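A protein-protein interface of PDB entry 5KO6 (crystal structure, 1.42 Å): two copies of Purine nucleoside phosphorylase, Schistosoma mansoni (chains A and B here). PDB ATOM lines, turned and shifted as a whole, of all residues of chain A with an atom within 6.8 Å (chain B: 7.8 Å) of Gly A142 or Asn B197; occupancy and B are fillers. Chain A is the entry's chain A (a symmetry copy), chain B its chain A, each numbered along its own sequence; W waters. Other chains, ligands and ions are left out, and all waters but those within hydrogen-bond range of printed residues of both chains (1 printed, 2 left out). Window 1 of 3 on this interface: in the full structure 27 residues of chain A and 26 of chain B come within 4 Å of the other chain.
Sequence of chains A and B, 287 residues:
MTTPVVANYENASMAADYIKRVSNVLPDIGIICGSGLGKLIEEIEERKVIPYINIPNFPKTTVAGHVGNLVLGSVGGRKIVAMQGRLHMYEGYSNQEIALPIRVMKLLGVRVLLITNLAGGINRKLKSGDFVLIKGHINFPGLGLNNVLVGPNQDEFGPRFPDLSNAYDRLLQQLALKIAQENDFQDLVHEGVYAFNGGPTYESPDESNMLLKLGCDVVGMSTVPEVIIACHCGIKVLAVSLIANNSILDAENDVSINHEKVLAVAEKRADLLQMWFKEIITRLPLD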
ATOM      1  N   ASN A 139      19.251  21.128 -17.752  1.00  0.00           N
ATOM      2  CA  ASN A 139      17.869  21.020 -17.280  1.00  0.00           C
ATOM      3  C   ASN A 139      17.880  20.204 -15.995  1.00  0.00           C
ATOM      4  O   ASN A 139      17.685  18.992 -16.012  1.00  0.00           O
ATOM      5  CB  ASN A 139      17.095  20.318 -18.393  1.00  0.00           C
ATOM      6  CG  ASN A 139      15.617  20.124 -18.109  1.00  0.00           C
ATOM      7  OD1 ASN A 139      15.051  20.634 -17.136  1.00  0.00           O
ATOM      8  ND2 ASN A 139      14.972  19.358 -18.992  1.00  0.00           N
ATOM      9  N   PHE A 140      18.091  20.874 -14.857  1.00  0.00           N
ATOM     10  CA  PHE A 140      18.114  20.140 -13.590  1.00  0.00           C
ATOM     11  C   PHE A 140      16.805  19.425 -13.321  1.00  0.00           C
ATOM     12  O   PHE A 140      16.840  18.242 -12.935  1.00  0.00           O
ATOM     13  CB  PHE A 140      18.568  21.046 -12.432  1.00  0.00           C
ATOM     14  CG  PHE A 140      20.007  21.443 -12.533  1.00  0.00           C
ATOM     15  CD1 PHE A 140      21.001  20.553 -12.160  1.00  0.00           C
ATOM     16  CD2 PHE A 140      20.369  22.676 -13.044  1.00  0.00           C
ATOM     17  CE1 PHE A 140      22.354  20.891 -12.266  1.00  0.00           C
ATOM     18  CE2 PHE A 140      21.714  23.020 -13.158  1.00  0.00           C
ATOM     19  CZ  PHE A 140      22.704  22.132 -12.766  1.00  0.00           C
ATOM     20  N   PRO A 141      15.635  20.037 -13.525  1.00  0.00           N
ATOM     21  CA  PRO A 141      14.397  19.266 -13.368  1.00  0.00           C
ATOM     22  C   PRO A 141      14.358  18.034 -14.254  1.00  0.00           C
ATOM     23  O   PRO A 141      13.942  16.966 -13.789  1.00  0.00           O
ATOM     24  CB  PRO A 141      13.308  20.286 -13.725  1.00  0.00           C
ATOM     25  CG  PRO A 141      13.931  21.624 -13.305  1.00  0.00           C
ATOM     26  CD  PRO A 141      15.356  21.468 -13.794  1.00  0.00           C
ATOM     27  N   GLY A 142      14.818  18.134 -15.504  1.00  0.00           N
ATOM     28  CA  GLY A 142      14.784  16.974 -16.388  1.00  0.00           C
ATOM     29  C   GLY A 142      15.686  15.848 -15.919  1.00  0.00           C
ATOM     30  O   GLY A 142      15.295  14.678 -15.910  1.00  0.00           O
ATOM     31  N   LEU A 143      16.915  16.173 -15.532  1.00  0.00           N
ATOM     32  CA  LEU A 143      17.756  15.129 -14.960  1.00  0.00           C
ATOM     33  C   LEU A 143      17.089  14.489 -13.748  1.00  0.00           C
ATOM     34  O   LEU A 143      17.223  13.280 -13.527  1.00  0.00           O
ATOM     35  CB  LEU A 143      19.132  15.695 -14.581  1.00  0.00           C
ATOM     36  CG  LEU A 143      19.979  16.188 -15.761  1.00  0.00           C
ATOM     37  CD1 LEU A 143      21.197  16.879 -15.225  1.00  0.00           C
ATOM     38  CD2 LEU A 143      20.395  15.016 -16.659  1.00  0.00           C
ATOM     39  N   GLY A 144      16.351  15.281 -12.962  1.00  0.00           N
ATOM     40  CA  GLY A 144      15.820  14.814 -11.690  1.00  0.00           C
ATOM     41  C   GLY A 144      14.396  14.290 -11.701  1.00  0.00           C
ATOM     42  O   GLY A 144      13.759  14.261 -10.647  1.00  0.00           O
ATOM     43  N   LEU A 145      13.891  13.821 -12.844  1.00  0.00           N
ATOM     44  CA  LEU A 145      12.572  13.175 -13.005  1.00  0.00           C
ATOM     45  C   LEU A 145      11.423  14.168 -13.022  1.00  0.00           C
ATOM     46  O   LEU A 145      10.260  13.746 -12.918  1.00  0.00           O
ATOM     47  CB  LEU A 145      12.287  12.007 -12.051  1.00  0.00           C
ATOM     48  CG  LEU A 145      12.555  10.617 -12.623  1.00  0.00           C
ATOM     49  CD1 LEU A 145      12.352   9.543 -11.561  1.00  0.00           C
ATOM     50  CD2 LEU A 145      11.646  10.325 -13.822  1.00  0.00           C
ATOM     51  N   ASN A 146      11.707  15.463 -13.201  1.00  0.00           N
ATOM     52  CA  ASN A 146      10.677  16.484 -13.385  1.00  0.00           C
ATOM     53  C   ASN A 146      10.724  17.109 -14.778  1.00  0.00           C
ATOM     54  O   ASN A 146      10.290  18.247 -14.965  1.00  0.00           O
ATOM     55  CB  ASN A 146      10.757  17.557 -12.291  1.00  0.00           C
ATOM     56  CG  ASN A 146      10.154  17.101 -10.979  1.00  0.00           C
ATOM     57  OD1 ASN A 146       9.297  16.212 -10.948  1.00  0.00           O
ATOM     58  ND2 ASN A 146      10.574  17.720  -9.888  1.00  0.00           N
ATOM     59  N   ASN A 147      11.233  16.385 -15.770  1.00  0.00           N
ATOM     60  CA  ASN A 147      11.162  16.875 -17.144  1.00  0.00           C
ATOM     61  C   ASN A 147       9.707  17.145 -17.507  1.00  0.00           C
ATOM     62  O   ASN A 147       8.804  16.413 -17.091  1.00  0.00           O
ATOM     63  CB  ASN A 147      11.738  15.782 -18.065  1.00  0.00           C
ATOM     64  CG  ASN A 147      12.034  16.260 -19.483  1.00  0.00           C
ATOM     65  OD1 ASN A 147      11.118  16.638 -20.226  1.00  0.00           O
ATOM     66  ND2 ASN A 147      13.309  16.183 -19.889  1.00  0.00           N
ATOM     67  N   VAL A 148       9.482  18.203 -18.299  1.00  0.00           N
ATOM     68  CA  VAL A 148       8.134  18.559 -18.732  1.00  0.00           C
ATOM     69  C   VAL A 148       7.469  17.459 -19.561  1.00  0.00           C
ATOM     70  O   VAL A 148       6.241  17.446 -19.669  1.00  0.00           O
ATOM     71  CB  VAL A 148       8.191  19.918 -19.472  1.00  0.00           C
ATOM     72  CG1 VAL A 148       8.878  19.743 -20.835  1.00  0.00           C
ATOM     73  CG2 VAL A 148       6.789  20.560 -19.634  1.00  0.00           C
ATOM     74  N   VAL A 150       7.714  14.132 -18.772  1.00  0.00           N
ATOM     75  CA  VAL A 150       7.382  12.946 -17.984  1.00  0.00           C
ATOM     76  C   VAL A 150       5.882  12.716 -18.042  1.00  0.00           C
ATOM     77  O   VAL A 150       5.087  13.641 -17.829  1.00  0.00           O
ATOM     78  CB  VAL A 150       7.884  13.103 -16.540  1.00  0.00           C
ATOM     79  CG1 VAL A 150       7.320  11.981 -15.641  1.00  0.00           C
ATOM     80  CG2 VAL A 150       9.395  13.068 -16.501  1.00  0.00           C
ATOM     81  N   PHE A 196      18.435  25.673 -15.958  1.00  0.00           N
ATOM     82  CA  PHE A 196      17.065  25.753 -15.457  1.00  0.00           C
ATOM     83  C   PHE A 196      17.061  25.412 -13.968  1.00  0.00           C
ATOM     84  O   PHE A 196      17.255  24.252 -13.588  1.00  0.00           O
ATOM     85  CB  PHE A 196      16.180  24.801 -16.256  1.00  0.00           C
ATOM     86  CG  PHE A 196      14.715  24.801 -15.858  1.00  0.00           C
ATOM     87  CD1 PHE A 196      14.128  25.876 -15.186  1.00  0.00           C
ATOM     88  CD2 PHE A 196      13.912  23.716 -16.188  1.00  0.00           C
ATOM     89  CE1 PHE A 196      12.778  25.849 -14.838  1.00  0.00           C
ATOM     90  CE2 PHE A 196      12.553  23.672 -15.846  1.00  0.00           C
ATOM     91  CZ  PHE A 196      11.982  24.753 -15.166  1.00  0.00           C
ATOM     92  N   VAL A 224      13.122  26.493 -20.483  1.00  0.00           N
ATOM     93  CA  VAL A 224      13.425  25.106 -20.858  1.00  0.00           C
ATOM     94  C   VAL A 224      12.170  24.264 -21.026  1.00  0.00           C
ATOM     95  O   VAL A 224      12.094  23.501 -22.001  1.00  0.00           O
ATOM     96  CB  VAL A 224      14.478  24.513 -19.904  1.00  0.00           C
ATOM     97  CG1 VAL A 224      14.586  22.980 -20.039  1.00  0.00           C
ATOM     98  CG2 VAL A 224      15.841  25.187 -20.116  1.00  0.00           C
ATOM     99  N   ILE A 228      11.337  22.492 -24.688  1.00  0.00           N
ATOM    100  CA  ILE A 228      11.237  21.050 -24.879  1.00  0.00           C
ATOM    101  C   ILE A 228       9.918  20.679 -25.545  1.00  0.00           C
ATOM    102  O   ILE A 228       9.891  19.855 -26.461  1.00  0.00           O
ATOM    103  CB  ILE A 228      11.463  20.327 -23.543  1.00  0.00           C
ATOM    104  CG1 ILE A 228      12.943  20.423 -23.149  1.00  0.00           C
ATOM    105  CG2 ILE A 228      11.014  18.868 -23.637  1.00  0.00           C
ATOM    106  CD1 ILE A 228      13.256  19.877 -21.745  1.00  0.00           C
ATOM    107  N   TYR B  90      10.084   7.781 -16.542  1.00  0.00           N
ATOM    108  CA  TYR B  90       9.667   8.868 -17.441  1.00  0.00           C
ATOM    109  C   TYR B  90       8.255   8.672 -17.980  1.00  0.00           C
ATOM    110  O   TYR B  90       7.695   9.614 -18.535  1.00  0.00           O
ATOM    111  CB  TYR B  90      10.651   9.101 -18.602  1.00  0.00           C
ATOM    112  CG  TYR B  90      10.899   7.879 -19.457  1.00  0.00           C
ATOM    113  CD1 TYR B  90       9.921   7.381 -20.306  1.00  0.00           C
ATOM    114  CD2 TYR B  90      12.130   7.241 -19.427  1.00  0.00           C
ATOM    115  CE1 TYR B  90      10.154   6.251 -21.076  1.00  0.00           C
ATOM    116  CE2 TYR B  90      12.367   6.108 -20.190  1.00  0.00           C
ATOM    117  CZ  TYR B  90      11.372   5.625 -21.008  1.00  0.00           C
ATOM    118  OH  TYR B  90      11.610   4.495 -21.767  1.00  0.00           O
ATOM    119  N   ILE B 138      25.140   7.894 -10.158  1.00  0.00           N
ATOM    120  CA  ILE B 138      24.792   9.245  -9.725  1.00  0.00           C
ATOM    121  C   ILE B 138      23.315   9.423 -10.022  1.00  0.00           C
ATOM    122  O   ILE B 138      22.898   9.416 -11.190  1.00  0.00           O
ATOM    123  CB  ILE B 138      25.644  10.320 -10.397  1.00  0.00           C
ATOM    124  CG1 ILE B 138      27.103  10.159  -9.961  1.00  0.00           C
ATOM    125  CG2 ILE B 138      25.148  11.716 -10.001  1.00  0.00           C
ATOM    126  CD1 ILE B 138      28.044  11.181 -10.550  1.00  0.00           C
ATOM    127  N   ASN B 139      22.520   9.524  -8.974  1.00  0.00           N
ATOM    128  CA  ASN B 139      21.059   9.443  -9.050  1.00  0.00           C
ATOM    129  C   ASN B 139      20.510  10.859  -8.942  1.00  0.00           C
ATOM    130  O   ASN B 139      20.160  11.322  -7.861  1.00  0.00           O
ATOM    131  CB  ASN B 139      20.622   8.572  -7.875  1.00  0.00           C
ATOM    132  CG  ASN B 139      19.125   8.342  -7.781  1.00  0.00           C
ATOM    133  OD1 ASN B 139      18.339   8.690  -8.670  1.00  0.00           O
ATOM    134  ND2 ASN B 139      18.719   7.735  -6.664  1.00  0.00           N
ATOM    135  N   PHE B 140      20.411  11.556 -10.079  1.00  0.00           N
ATOM    136  CA  PHE B 140      19.892  12.923 -10.036  1.00  0.00           C
ATOM    137  C   PHE B 140      18.481  12.980  -9.484  1.00  0.00           C
ATOM    138  O   PHE B 140      18.210  13.843  -8.629  1.00  0.00           O
ATOM    139  CB  PHE B 140      20.046  13.620 -11.400  1.00  0.00           C
ATOM    140  CG  PHE B 140      21.474  13.892 -11.757  1.00  0.00           C
ATOM    141  CD1 PHE B 140      22.139  14.966 -11.189  1.00  0.00           C
ATOM    142  CD2 PHE B 140      22.164  13.052 -12.612  1.00  0.00           C
ATOM    143  CE1 PHE B 140      23.480  15.228 -11.487  1.00  0.00           C
ATOM    144  CE2 PHE B 140      23.501  13.302 -12.912  1.00  0.00           C
ATOM    145  CZ  PHE B 140      24.156  14.390 -12.355  1.00  0.00           C
ATOM    146  N   PRO B 141      17.554  12.104  -9.881  1.00  0.00           N
ATOM    147  CA  PRO B 141      16.240  12.122  -9.229  1.00  0.00           C
ATOM    148  C   PRO B 141      16.330  11.948  -7.724  1.00  0.00           C
ATOM    149  O   PRO B 141      15.630  12.655  -6.989  1.00  0.00           O
ATOM    150  CB  PRO B 141      15.499  10.967  -9.915  1.00  0.00           C
ATOM    151  CG  PRO B 141      16.127  10.930 -11.315  1.00  0.00           C
ATOM    152  CD  PRO B 141      17.594  11.133 -11.000  1.00  0.00           C
ATOM    153  N   ASN B 146      13.136  12.985  -5.860  1.00  0.00           N
ATOM    154  CA  ASN B 146      12.391  11.991  -6.631  1.00  0.00           C
ATOM    155  C   ASN B 146      13.005  10.596  -6.522  1.00  0.00           C
ATOM    156  O   ASN B 146      12.830   9.767  -7.417  1.00  0.00           O
ATOM    157  CB  ASN B 146      12.246  12.420  -8.097  1.00  0.00           C
ATOM    158  CG  ASN B 146      11.169  13.467  -8.295  1.00  0.00           C
ATOM    159  OD1 ASN B 146      10.234  13.578  -7.495  1.00  0.00           O
ATOM    160  ND2 ASN B 146      11.273  14.226  -9.373  1.00  0.00           N
ATOM    161  N   TYR B 194      27.110   5.042 -13.633  1.00  0.00           N
ATOM    162  CA  TYR B 194      25.903   5.328 -14.407  1.00  0.00           C
ATOM    163  C   TYR B 194      25.195   6.564 -13.853  1.00  0.00           C
ATOM    164  O   TYR B 194      24.804   6.587 -12.684  1.00  0.00           O
ATOM    165  CB  TYR B 194      24.971   4.119 -14.329  1.00  0.00           C
ATOM    166  CG  TYR B 194      23.663   4.183 -15.097  1.00  0.00           C
ATOM    167  CD1 TYR B 194      22.533   4.796 -14.539  1.00  0.00           C
ATOM    168  CD2 TYR B 194      23.529   3.559 -16.345  1.00  0.00           C
ATOM    169  CE1 TYR B 194      21.330   4.814 -15.219  1.00  0.00           C
ATOM    170  CE2 TYR B 194      22.327   3.566 -17.035  1.00  0.00           C
ATOM    171  CZ  TYR B 194      21.227   4.204 -16.464  1.00  0.00           C
ATOM    172  OH  TYR B 194      20.037   4.204 -17.129  1.00  0.00           O
ATOM    173  N   ALA B 195      24.980   7.560 -14.705  1.00  0.00           N
ATOM    174  CA  ALA B 195      24.162   8.715 -14.336  1.00  0.00           C
ATOM    175  C   ALA B 195      22.721   8.457 -14.743  1.00  0.00           C
ATOM    176  O   ALA B 195      22.446   8.131 -15.901  1.00  0.00           O
ATOM    177  CB  ALA B 195      24.647   9.966 -15.063  1.00  0.00           C
ATOM    178  N   PHE B 196      21.803   8.614 -13.790  1.00  0.00           N
ATOM    179  CA  PHE B 196      20.371   8.476 -14.046  1.00  0.00           C
ATOM    180  C   PHE B 196      19.807   9.836 -14.452  1.00  0.00           C
ATOM    181  O   PHE B 196      19.689  10.742 -13.620  1.00  0.00           O
ATOM    182  CB  PHE B 196      19.687   7.932 -12.796  1.00  0.00           C
ATOM    183  CG  PHE B 196      18.191   7.712 -12.928  1.00  0.00           C
ATOM    184  CD1 PHE B 196      17.571   7.551 -14.169  1.00  0.00           C
ATOM    185  CD2 PHE B 196      17.402   7.639 -11.786  1.00  0.00           C
ATOM    186  CE1 PHE B 196      16.195   7.345 -14.259  1.00  0.00           C
ATOM    187  CE2 PHE B 196      16.017   7.432 -11.857  1.00  0.00           C
ATOM    188  CZ  PHE B 196      15.410   7.281 -13.108  1.00  0.00           C
ATOM    189  N   ASN B 197      19.500   9.976 -15.746  1.00  0.00           N
ATOM    190  CA  ASN B 197      18.721  11.084 -16.289  1.00  0.00           C
ATOM    191  C   ASN B 197      17.266  10.639 -16.332  1.00  0.00           C
ATOM    192  O   ASN B 197      16.923   9.701 -17.056  1.00  0.00           O
ATOM    193  CB  ASN B 197      19.208  11.367 -17.714  1.00  0.00           C
ATOM    194  CG  ASN B 197      18.270  12.276 -18.489  1.00  0.00           C
ATOM    195  OD1 ASN B 197      17.586  13.123 -17.913  1.00  0.00           O
ATOM    196  ND2 ASN B 197      18.234  12.096 -19.819  1.00  0.00           N
ATOM    197  N   GLY B 198      16.409  11.305 -15.552  1.00  0.00           N
ATOM    198  CA  GLY B 198      15.013  10.892 -15.508  1.00  0.00           C
ATOM    199  C   GLY B 198      14.368  10.771 -16.878  1.00  0.00           C
ATOM    200  O   GLY B 198      13.525   9.892 -17.100  1.00  0.00           O
ATOM    201  N   GLY B 199      14.725  11.660 -17.803  1.00  0.00           N
ATOM    202  CA  GLY B 199      14.218  11.566 -19.166  1.00  0.00           C
ATOM    203  C   GLY B 199      12.838  12.199 -19.327  1.00  0.00           C
ATOM    204  O   GLY B 199      12.314  12.804 -18.410  1.00  0.00           O
ATOM    205  N   PRO B 200      12.195  12.033 -20.489  1.00  0.00           N
ATOM    206  CA  PRO B 200      12.555  11.131 -21.594  1.00  0.00           C
ATOM    207  C   PRO B 200      13.370  11.788 -22.700  1.00  0.00           C
ATOM    208  O   PRO B 200      13.705  11.077 -23.663  1.00  0.00           O
ATOM    209  CB  PRO B 200      11.184  10.743 -22.162  1.00  0.00           C
ATOM    210  CG  PRO B 200      10.360  12.014 -21.970  1.00  0.00           C
ATOM    211  CD  PRO B 200      10.841  12.589 -20.636  1.00  0.00           C
ATOM    212  N   THR B 201      13.683  13.081 -22.612  1.00  0.00           N
ATOM    213  CA  THR B 201      14.617  13.654 -23.580  1.00  0.00           C
ATOM    214  C   THR B 201      16.020  13.126 -23.309  1.00  0.00           C
ATOM    215  O   THR B 201      16.447  12.992 -22.157  1.00  0.00           O
ATOM    216  CB  THR B 201      14.625  15.180 -23.513  1.00  0.00           C
ATOM    217  OG1 THR B 201      14.912  15.608 -22.173  1.00  0.00           O
ATOM    218  CG2 THR B 201      13.275  15.756 -23.925  1.00  0.00           C
ATOM    219  N   TYR B 202      16.741  12.804 -24.380  1.00  0.00           N
ATOM    220  CA  TYR B 202      18.142  12.455 -24.234  1.00  0.00           C
ATOM    221  C   TYR B 202      18.889  13.609 -23.583  1.00  0.00           C
ATOM    222  O   TYR B 202      18.486  14.776 -23.692  1.00  0.00           O
ATOM    223  CB  TYR B 202      18.760  12.163 -25.610  1.00  0.00           C
ATOM    224  CG  TYR B 202      18.186  10.916 -26.251  1.00  0.00           C
ATOM    225  CD1 TYR B 202      18.468   9.661 -25.725  1.00  0.00           C
ATOM    226  CD2 TYR B 202      17.352  10.994 -27.359  1.00  0.00           C
ATOM    227  CE1 TYR B 202      17.946   8.515 -26.294  1.00  0.00           C
ATOM    228  CE2 TYR B 202      16.824   9.851 -27.918  1.00  0.00           C
ATOM    229  CZ  TYR B 202      17.133   8.627 -27.378  1.00  0.00           C
ATOM    230  OH  TYR B 202      16.602   7.485 -27.929  1.00  0.00           O
ATOM    231  N   GLU B 203      19.967  13.267 -22.880  1.00  0.00           N
ATOM    232  CA  GLU B 203      20.851  14.278 -22.317  1.00  0.00           C
ATOM    233  C   GLU B 203      21.224  15.277 -23.404  1.00  0.00           C
ATOM    234  O   GLU B 203      21.548  14.896 -24.533  1.00  0.00           O
ATOM    235  CB  GLU B 203      22.118  13.581 -21.768  1.00  0.00           C
ATOM    236  CG  GLU B 203      23.055  12.859 -22.799  1.00  0.00           C
ATOM    237  CD  GLU B 203      22.617  11.469 -23.237  1.00  0.00           C
ATOM    238  OE1 GLU B 203      21.526  11.019 -22.862  1.00  0.00           O
ATOM    239  OE2 GLU B 203      23.373  10.798 -23.981  1.00  0.00           O
ATOM    240  N   SER B 204      21.106  16.569 -23.079  1.00  0.00           N
ATOM    241  CA  SER B 204      21.492  17.605 -24.021  1.00  0.00           C
ATOM    242  C   SER B 204      23.012  17.642 -24.132  1.00  0.00           C
ATOM    243  O   SER B 204      23.713  17.132 -23.254  1.00  0.00           O
ATOM    244  CB  SER B 204      20.997  18.960 -23.531  1.00  0.00           C
ATOM    245  OG  SER B 204      21.782  19.416 -22.440  1.00  0.00           O
ATOM    246  N   GLU B 207      24.404  19.062 -21.060  1.00  0.00           N
ATOM    247  CA  GLU B 207      24.293  18.125 -19.948  1.00  0.00           C
ATOM    248  C   GLU B 207      25.354  17.034 -20.046  1.00  0.00           C
ATOM    249  O   GLU B 207      25.946  16.642 -19.033  1.00  0.00           O
ATOM    250  CB  GLU B 207      22.892  17.519 -19.910  1.00  0.00           C
ATOM    251  CG  GLU B 207      21.845  18.536 -19.428  1.00  0.00           C
ATOM    252  CD  GLU B 207      20.422  18.205 -19.868  1.00  0.00           C
ATOM    253  OE1 GLU B 207      20.178  17.106 -20.415  1.00  0.00           O
ATOM    254  OE2 GLU B 207      19.534  19.063 -19.694  1.00  0.00           O
ATOM    255  N   LEU B 211      28.099  16.030 -17.266  1.00  0.00           N
ATOM    256  CA  LEU B 211      28.259  14.690 -16.699  1.00  0.00           C
ATOM    257  C   LEU B 211      29.705  14.225 -16.755  1.00  0.00           C
ATOM    258  O   LEU B 211      30.178  13.520 -15.852  1.00  0.00           O
ATOM    259  CB  LEU B 211      27.351  13.699 -17.420  1.00  0.00           C
ATOM    260  CG  LEU B 211      25.869  13.974 -17.242  1.00  0.00           C
ATOM    261  CD1 LEU B 211      25.068  12.925 -17.985  1.00  0.00           C
ATOM    262  CD2 LEU B 211      25.501  13.975 -15.759  1.00  0.00           C
ATOM    263  N   VAL B 218      28.531   6.747 -18.105  1.00  0.00           N
ATOM    264  CA  VAL B 218      27.408   6.479 -18.996  1.00  0.00           C
ATOM    265  C   VAL B 218      26.198   7.195 -18.412  1.00  0.00           C
ATOM    266  O   VAL B 218      26.193   7.580 -17.242  1.00  0.00           O
ATOM    267  CB  VAL B 218      27.095   4.973 -19.168  1.00  0.00           C
ATOM    268  CG1 VAL B 218      28.331   4.201 -19.571  1.00  0.00           C
ATOM    269  CG2 VAL B 218      26.524   4.392 -17.905  1.00  0.00           C
ATOM    270  N   VAL B 219      25.169   7.385 -19.240  1.00  0.00           N
ATOM    271  CA  VAL B 219      23.944   8.065 -18.815  1.00  0.00           C
ATOM    272  C   VAL B 219      22.751   7.354 -19.440  1.00  0.00           C
ATOM    273  O   VAL B 219      22.780   6.975 -20.616  1.00  0.00           O
ATOM    274  CB  VAL B 219      23.967   9.567 -19.179  1.00  0.00           C
ATOM    275  CG1 VAL B 219      24.171   9.768 -20.680  1.00  0.00           C
ATOM    276  CG2 VAL B 219      22.689  10.256 -18.719  1.00  0.00           C
ATOM    277  N   GLY B 220      21.706   7.150 -18.647  1.00  0.00           N
ATOM    278  CA  GLY B 220      20.506   6.519 -19.166  1.00  0.00           C
ATOM    279  C   GLY B 220      19.320   6.849 -18.291  1.00  0.00           C
ATOM    280  O   GLY B 220      19.443   7.564 -17.288  1.00  0.00           O
ATOM    281  N   MET B 221      18.161   6.298 -18.661  1.00  0.00           N
ATOM    282  CA  MET B 221      16.879   6.701 -18.083  1.00  0.00           C
ATOM    283  C   MET B 221      16.219   5.590 -17.282  1.00  0.00           C
ATOM    284  O   MET B 221      15.001   5.615 -17.082  1.00  0.00           O
ATOM    285  CB  MET B 221      15.929   7.172 -19.187  1.00  0.00           C
ATOM    286  CG  MET B 221      16.547   8.162 -20.137  1.00  0.00           C
ATOM    287  SD  MET B 221      15.359   8.568 -21.446  1.00  0.00           S
ATOM    288  CE  MET B 221      16.413   9.485 -22.536  1.00  0.00           C
ATOM    289  N   SER B 222      16.983   4.599 -16.842  1.00  0.00           N
ATOM    290  CA  SER B 222      16.385   3.454 -16.175  1.00  0.00           C
ATOM    291  C   SER B 222      17.345   2.965 -15.100  1.00  0.00           C
ATOM    292  O   SER B 222      18.305   3.654 -14.728  1.00  0.00           O
ATOM    293  CB  SER B 222      16.081   2.341 -17.187  1.00  0.00           C
ATOM    294  OG  SER B 222      17.288   1.748 -17.638  1.00  0.00           O
ATOM    295  N   VAL B 224      18.547   2.605 -12.160  1.00  0.00           N
ATOM    296  CA  VAL B 224      18.756   3.043 -10.774  1.00  0.00           C
ATOM    297  C   VAL B 224      17.527   2.823  -9.905  1.00  0.00           C
ATOM    298  O   VAL B 224      17.681   2.351  -8.769  1.00  0.00           O
ATOM    299  CB  VAL B 224      19.319   4.476 -10.746  1.00  0.00           C
ATOM    300  CG1 VAL B 224      19.244   5.101  -9.338  1.00  0.00           C
ATOM    301  CG2 VAL B 224      20.755   4.503 -11.290  1.00  0.00           C
HETATM  302  O   HOH W   1      17.184  18.713 -21.056  1.00  0.00           O
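ND2 of Asn B146 is in hydrogen-bond range of OD1 of Asn A146 (3.2 Å). The side-chain amide nitrogen of Asn B146 lies within hydrogen-bond range of the backbone carbonyl oxygen of Gly A144, at 2.8 Å. The backbone carbonyl oxygen of Leu A143 lies within hydrogen-bond range of the backbone NH of Gly B198. The side-chain carboxylate of Glu B207 is in hydrogen-bond range of the backbone NH of Asn A139 (2.8 Å). The side-chain amide oxygen (OD1) of Asn B197 sits close to the backbone carbonyl oxygen (O) of Gly A142, 3.4 Å away. OG1 of Thr B201 is in hydrogen-bond range of ND2 of Asn A147.
The backbone carbonyl oxygen (O) of Pro B141 is in hydrogen-bond range of the backbone NH (N) of Asn B146. OD1 of Asn B197 sits close to N of Gly B199 (3.2 Å). O of Gly B220 lies within hydrogen-bond range of N of Asn B197 (2.9 Å). N of Gly A142 is in hydrogen-bond range of OD1 of Asn A139, 3.0 Å away.
Gly B198 touches Gly A142. Pro B141 touches Leu A143 (CD to O, 3.3 Å). CA of Leu A143 touches OD1 of Asn B197, 3.6 Å away. Gly A144 touches Phe B140. CA of Pro B141 touches O of Gly A144, 3.6 Å away. Leu A145 touches Pro B141. Leu A145 touches Gly B198 (CG to CA, 3.8 Å). O of Gly B199 touches CB of Asn A147 (3.1 Å). Val A150 touches Tyr B90 (CA to O, 3.4 Å).
Of chain B, only Asn B197 (3.4 Å), Gly B198 (3.6 Å) and Gly B199 (3.6 Å) come within 4 Å of Gly A142. Asn B197 touches just these residues of chain A: Gly A142 (3.4 Å) and Leu A143 (3.6 Å). Printed residues of chain B within 4 Å of Val A150: Tyr B90 (3.4 Å), Gly B199 (3.5 Å) and Pro B200 (3.95 Å). Of the printed residues of chain A, Pro B200 touches Val A150. Of the printed residues of chain A, Asn B146 touches Gly A144, Leu A145 and Asn A146. Phe A196 touches none of the printed residues of chain B. Phe A140 touches none of the printed residues of chain B. The nearest residue of chain B that does not touch Gly A142 is Thr B201 (5.9 Å). The nearest residue of chain A that does not touch Asn B197 is Gly A144 (5.5 Å). The nearest printed residue of chain A that does not touch Glu B207 is Leu A143 (4.3 Å).
Hydrophobic or aromatic side chains of chain B that line the printed part of chain A: Phe B140, Pro B141 and Pro B200. Of the 14 printed residues of chain A, 9 touch a printed residue of chain B. Printed residues of chain A that touch a printed residue of chain B: Asn A139, Gly A142, Leu A143, Gly A144, Leu A145, Asn A146, Asn A147, Val A150 and Ile A228. Hydrophobic or aromatic side chains of chain A within 4 Å of the printed part of chain B: Leu A143, Leu A145, Val A150 and Ile A228. Among the printed residues, 22 pairs touch across the chains. Among the printed residues, no Asp or Glu carboxylate lies within 4 Å of a Lys or Arg side-chain nitrogen of the other chain.
Asn A146 touches its own counterpart, Asn B146.
Water W1 bridges the side-chain carboxylate (OE2) of Glu B207 and the side-chain amide nitrogen (ND2) of Asn A139.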
